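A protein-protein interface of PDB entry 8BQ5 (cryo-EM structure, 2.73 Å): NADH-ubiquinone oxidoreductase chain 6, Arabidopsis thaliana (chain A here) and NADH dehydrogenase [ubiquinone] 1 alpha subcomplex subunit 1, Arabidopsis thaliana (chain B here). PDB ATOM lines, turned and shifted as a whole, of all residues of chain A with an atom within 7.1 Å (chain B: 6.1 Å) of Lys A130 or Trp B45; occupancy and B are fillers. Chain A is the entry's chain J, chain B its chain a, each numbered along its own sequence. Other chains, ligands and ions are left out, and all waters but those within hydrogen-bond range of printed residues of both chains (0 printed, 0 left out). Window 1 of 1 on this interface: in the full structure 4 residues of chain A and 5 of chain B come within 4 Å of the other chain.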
ATOM      1  N   THR A 125      35.047   6.941   0.952  1.00  0.00           N
ATOM      2  CA  THR A 125      34.502   6.451   2.250  1.00  0.00           C
ATOM      3  C   THR A 125      34.568   4.924   2.328  1.00  0.00           C
ATOM      4  O   THR A 125      34.036   4.253   1.433  1.00  0.00           O
ATOM      5  CB  THR A 125      33.074   6.962   2.466  1.00  0.00           C
ATOM      6  OG1 THR A 125      33.140   8.381   2.602  1.00  0.00           O
ATOM      7  CG2 THR A 125      32.392   6.367   3.679  1.00  0.00           C
ATOM      8  N   VAL A 126      35.205   4.399   3.373  1.00  0.00           N
ATOM      9  CA  VAL A 126      35.332   2.960   3.563  1.00  0.00           C
ATOM     10  C   VAL A 126      34.399   2.565   4.697  1.00  0.00           C
ATOM     11  O   VAL A 126      34.569   3.013   5.838  1.00  0.00           O
ATOM     12  CB  VAL A 126      36.780   2.552   3.864  1.00  0.00           C
ATOM     13  CG1 VAL A 126      36.910   1.039   3.893  1.00  0.00           C
ATOM     14  CG2 VAL A 126      37.714   3.153   2.833  1.00  0.00           C
ATOM     15  N   TYR A 127      33.412   1.723   4.394  1.00  0.00           N
ATOM     16  CA  TYR A 127      32.444   1.323   5.404  1.00  0.00           C
ATOM     17  C   TYR A 127      32.938   0.183   6.282  1.00  0.00           C
ATOM     18  O   TYR A 127      32.297  -0.121   7.292  1.00  0.00           O
ATOM     19  CB  TYR A 127      31.125   0.918   4.745  1.00  0.00           C
ATOM     20  CG  TYR A 127      30.418   2.063   4.069  1.00  0.00           C
ATOM     21  CD1 TYR A 127      29.591   2.911   4.788  1.00  0.00           C
ATOM     22  CD2 TYR A 127      30.577   2.296   2.712  1.00  0.00           C
ATOM     23  CE1 TYR A 127      28.945   3.959   4.176  1.00  0.00           C
ATOM     24  CE2 TYR A 127      29.934   3.342   2.090  1.00  0.00           C
ATOM     25  CZ  TYR A 127      29.119   4.170   2.827  1.00  0.00           C
ATOM     26  OH  TYR A 127      28.473   5.216   2.217  1.00  0.00           O
ATOM     27  N   ALA A 128      34.051  -0.457   5.918  1.00  0.00           N
ATOM     28  CA  ALA A 128      34.520  -1.609   6.681  1.00  0.00           C
ATOM     29  C   ALA A 128      34.961  -1.206   8.083  1.00  0.00           C
ATOM     30  O   ALA A 128      34.664  -1.904   9.059  1.00  0.00           O
ATOM     31  CB  ALA A 128      35.654  -2.304   5.933  1.00  0.00           C
ATOM     32  N   GLY A 129      35.661  -0.082   8.205  1.00  0.00           N
ATOM     33  CA  GLY A 129      36.080   0.393   9.509  1.00  0.00           C
ATOM     34  C   GLY A 129      35.007   1.092  10.309  1.00  0.00           C
ATOM     35  O   GLY A 129      35.262   1.477  11.454  1.00  0.00           O
ATOM     36  N   LYS A 130      33.814   1.267   9.745  1.00  0.00           N
ATOM     37  CA  LYS A 130      32.714   1.936  10.421  1.00  0.00           C
ATOM     38  C   LYS A 130      31.670   0.971  10.960  1.00  0.00           C
ATOM     39  O   LYS A 130      30.667   1.418  11.521  1.00  0.00           O
ATOM     40  CB  LYS A 130      32.042   2.929   9.472  1.00  0.00           C
ATOM     41  CG  LYS A 130      32.775   4.239   9.311  1.00  0.00           C
ATOM     42  CD  LYS A 130      32.177   5.045   8.174  1.00  0.00           C
ATOM     43  CE  LYS A 130      33.149   6.094   7.671  1.00  0.00           C
ATOM     44  NZ  LYS A 130      32.743   7.464   8.080  1.00  0.00           N
ATOM     45  N   VAL A 131      31.869  -0.337  10.791  1.00  0.00           N
ATOM     46  CA  VAL A 131      30.877  -1.302  11.254  1.00  0.00           C
ATOM     47  C   VAL A 131      30.824  -1.321  12.774  1.00  0.00           C
ATOM     48  O   VAL A 131      29.744  -1.279  13.375  1.00  0.00           O
ATOM     49  CB  VAL A 131      31.188  -2.694  10.680  1.00  0.00           C
ATOM     50  CG1 VAL A 131      30.257  -3.734  11.276  1.00  0.00           C
ATOM     51  CG2 VAL A 131      31.090  -2.674   9.170  1.00  0.00           C
ATOM     52  N   ARG A 132      31.988  -1.390  13.418  1.00  0.00           N
ATOM     53  CA  ARG A 132      32.116  -1.324  14.875  1.00  0.00           C
ATOM     54  C   ARG A 132      33.182  -0.271  15.165  1.00  0.00           C
ATOM     55  O   ARG A 132      34.369  -0.491  14.918  1.00  0.00           O
ATOM     56  CB  ARG A 132      32.479  -2.675  15.474  1.00  0.00           C
ATOM     57  CG  ARG A 132      32.736  -2.627  16.970  1.00  0.00           C
ATOM     58  CD  ARG A 132      33.050  -4.003  17.527  1.00  0.00           C
ATOM     59  NE  ARG A 132      33.281  -3.966  18.966  1.00  0.00           N
ATOM     60  CZ  ARG A 132      33.330  -5.037  19.746  1.00  0.00           C
ATOM     61  NH1 ARG A 132      33.150  -6.255  19.261  1.00  0.00           N
ATOM     62  NH2 ARG A 132      33.562  -4.883  21.046  1.00  0.00           N
ATOM     63  N   SER A 133      32.750   0.869  15.689  1.00  0.00           N
ATOM     64  CA  SER A 133      33.669   1.958  15.977  1.00  0.00           C
ATOM     65  C   SER A 133      34.187   1.871  17.407  1.00  0.00           C
ATOM     66  O   SER A 133      33.438   1.569  18.339  1.00  0.00           O
ATOM     67  CB  SER A 133      32.983   3.302  15.746  1.00  0.00           C
ATOM     68  OG  SER A 133      31.656   3.288  16.243  1.00  0.00           O
ATOM     69  N   ASP B  43      26.469   6.681  15.685  1.00  0.00           N
ATOM     70  CA  ASP B  43      27.901   6.506  15.501  1.00  0.00           C
ATOM     71  C   ASP B  43      28.302   6.887  14.078  1.00  0.00           C
ATOM     72  O   ASP B  43      27.505   7.436  13.310  1.00  0.00           O
ATOM     73  CB  ASP B  43      28.313   5.071  15.852  1.00  0.00           C
ATOM     74  CG  ASP B  43      27.475   4.018  15.146  1.00  0.00           C
ATOM     75  OD1 ASP B  43      27.003   4.262  14.016  1.00  0.00           O
ATOM     76  OD2 ASP B  43      27.295   2.928  15.729  1.00  0.00           O
ATOM     77  N   GLU B  44      29.566   6.612  13.738  1.00  0.00           N
ATOM     78  CA  GLU B  44      30.068   6.915  12.400  1.00  0.00           C
ATOM     79  C   GLU B  44      29.204   6.266  11.325  1.00  0.00           C
ATOM     80  O   GLU B  44      28.951   6.865  10.272  1.00  0.00           O
ATOM     81  CB  GLU B  44      31.518   6.446  12.259  1.00  0.00           C
ATOM     82  CG  GLU B  44      32.561   7.280  12.996  1.00  0.00           C
ATOM     83  CD  GLU B  44      32.367   7.286  14.502  1.00  0.00           C
ATOM     84  OE1 GLU B  44      32.177   6.204  15.090  1.00  0.00           O
ATOM     85  OE2 GLU B  44      32.414   8.375  15.101  1.00  0.00           O
ATOM     86  N   TRP B  45      28.741   5.039  11.575  1.00  0.00           N
ATOM     87  CA  TRP B  45      27.936   4.326  10.589  1.00  0.00           C
ATOM     88  C   TRP B  45      26.591   5.007  10.372  1.00  0.00           C
ATOM     89  O   TRP B  45      26.146   5.170   9.232  1.00  0.00           O
ATOM     90  CB  TRP B  45      27.739   2.875  11.023  1.00  0.00           C
ATOM     91  CG  TRP B  45      26.932   2.064  10.056  1.00  0.00           C
ATOM     92  CD1 TRP B  45      25.572   1.987   9.984  1.00  0.00           C
ATOM     93  CD2 TRP B  45      27.438   1.210   9.025  1.00  0.00           C
ATOM     94  NE1 TRP B  45      25.200   1.140   8.971  1.00  0.00           N
ATOM     95  CE2 TRP B  45      26.327   0.651   8.365  1.00  0.00           C
ATOM     96  CE3 TRP B  45      28.721   0.865   8.593  1.00  0.00           C
ATOM     97  CZ2 TRP B  45      26.461  -0.236   7.300  1.00  0.00           C
ATOM     98  CZ3 TRP B  45      28.852  -0.013   7.536  1.00  0.00           C
ATOM     99  CH2 TRP B  45      27.729  -0.553   6.900  1.00  0.00           C
ATOM    100  N   ASP B  46      25.917   5.398  11.457  1.00  0.00           N
ATOM    101  CA  ASP B  46      24.629   6.072  11.321  1.00  0.00           C
ATOM    102  C   ASP B  46      24.778   7.402  10.591  1.00  0.00           C
ATOM    103  O   ASP B  46      23.938   7.760   9.756  1.00  0.00           O
ATOM    104  CB  ASP B  46      23.994   6.278  12.697  1.00  0.00           C
ATOM    105  CG  ASP B  46      23.539   4.977  13.332  1.00  0.00           C
ATOM    106  OD1 ASP B  46      22.875   4.174  12.644  1.00  0.00           O
ATOM    107  OD2 ASP B  46      23.850   4.754  14.519  1.00  0.00           O
ATOM    108  N   VAL B  47      25.862   8.129  10.856  1.00  0.00           N
ATOM    109  CA  VAL B  47      26.111   9.421  10.150  1.00  0.00           C
ATOM    110  C   VAL B  47      26.337   9.166   8.653  1.00  0.00           C
ATOM    111  O   VAL B  47      25.691   9.851   7.847  1.00  0.00           O
ATOM    112  CB  VAL B  47      27.277  10.180  10.811  1.00  0.00           C
ATOM    113  CG1 VAL B  47      27.782  11.329   9.958  1.00  0.00           C
ATOM    114  CG2 VAL B  47      26.890  10.669  12.197  1.00  0.00           C
ATOM    115  N   ALA B  48      27.200   8.213   8.297  1.00  0.00           N
ATOM    116  CA  ALA B  48      27.465   7.865   6.880  1.00  0.00           C
ATOM    117  C   ALA B  48      26.155   7.489   6.179  1.00  0.00           C
ATOM    118  O   ALA B  48      25.949   7.951   5.049  1.00  0.00           O
ATOM    119  CB  ALA B  48      28.468   6.743   6.816  1.00  0.00           C
ATOM    120  N   MET B  49      25.288   6.733   6.849  1.00  0.00           N
ATOM    121  CA  MET B  49      23.984   6.322   6.266  1.00  0.00           C
ATOM    122  C   MET B  49      23.138   7.558   5.962  1.00  0.00           C
ATOM    123  O   MET B  49      22.683   7.664   4.830  1.00  0.00           O
ATOM    124  CB  MET B  49      23.224   5.416   7.236  1.00  0.00           C
ATOM    125  CG  MET B  49      23.751   4.002   7.308  1.00  0.00           C
ATOM    126  SD  MET B  49      24.269   3.357   5.709  1.00  0.00           S
ATOM    127  CE  MET B  49      26.042   3.299   5.947  1.00  0.00           C
ATOM    128  N   GLU B  50      22.952   8.446   6.939  1.00  0.00           N
ATOM    129  CA  GLU B  50      22.121   9.665   6.770  1.00  0.00           C
ATOM    130  C   GLU B  50      22.597  10.499   5.574  1.00  0.00           C
ATOM    131  O   GLU B  50      21.740  10.913   4.776  1.00  0.00           O
ATOM    132  CB  GLU B  50      22.201  10.500   8.041  1.00  0.00           C
ATOM    133  CG  GLU B  50      21.150  10.140   9.073  1.00  0.00           C
ATOM    134  CD  GLU B  50      21.020  11.130  10.218  1.00  0.00           C
ATOM    135  OE1 GLU B  50      20.166  10.902  11.096  1.00  0.00           O
ATOM    136  OE2 GLU B  50      21.774  12.127  10.233  1.00  0.00           O
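The side-chain hydroxyl of Ser A133 sits close to the side-chain carboxylate of Glu B44 (3.2 Å).
The side-chain carboxylate (OD1) of Asp B43 is in hydrogen-bond range of the backbone NH (N) of Trp B45 (3.1 Å).
The side-chain carboxylate (OD1) of Asp B43 lies within hydrogen-bond range of the backbone NH (N) of Asp B46 (3.0 Å).
Trp B45 touches Tyr A127.
CE1 of Tyr A127 touches CB of Ala B48 (3.9 Å).
Tyr A127 touches Met B49 (CE1 to CE, 3.5 Å).
Glu B44 touches Lys A130.
Lys A130 touches Trp B45 (O to CB, 3.3 Å).
Val A131 touches Trp B45.
Ser A133 touches Asp B43 (OG to CB, 3.8 Å).
Of the printed residues of chain B, Lys A130 touches Glu B44 (3.9 Å) and Trp B45 (3.3 Å).
Of the printed residues of chain A, Asp B43 touches Ser A133 (3.8 Å).
Of the printed residues of chain A, Glu B44 touches Lys A130 and Ser A133.
Of the printed residues of chain A, Ala B48 touches Tyr A127 (3.9 Å).
Of the printed residues of chain A, Met B49 touches Tyr A127 (3.5 Å).
The nearest residue of chain A that does not touch Trp B45 is Ala A128 (5.5 Å).
Of the 9 printed residues of chain A, 4 touch a printed residue of chain B.
Printed residues of chain A that touch a printed residue of chain B: Tyr A127, Lys A130, Val A131 and Ser A133.
Hydrophobic or aromatic side chains of chain A within 4 Å of the printed part of chain B: Tyr A127 and Val A131.
Of the 8 printed residues of chain B, 5 touch a printed residue of chain A.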
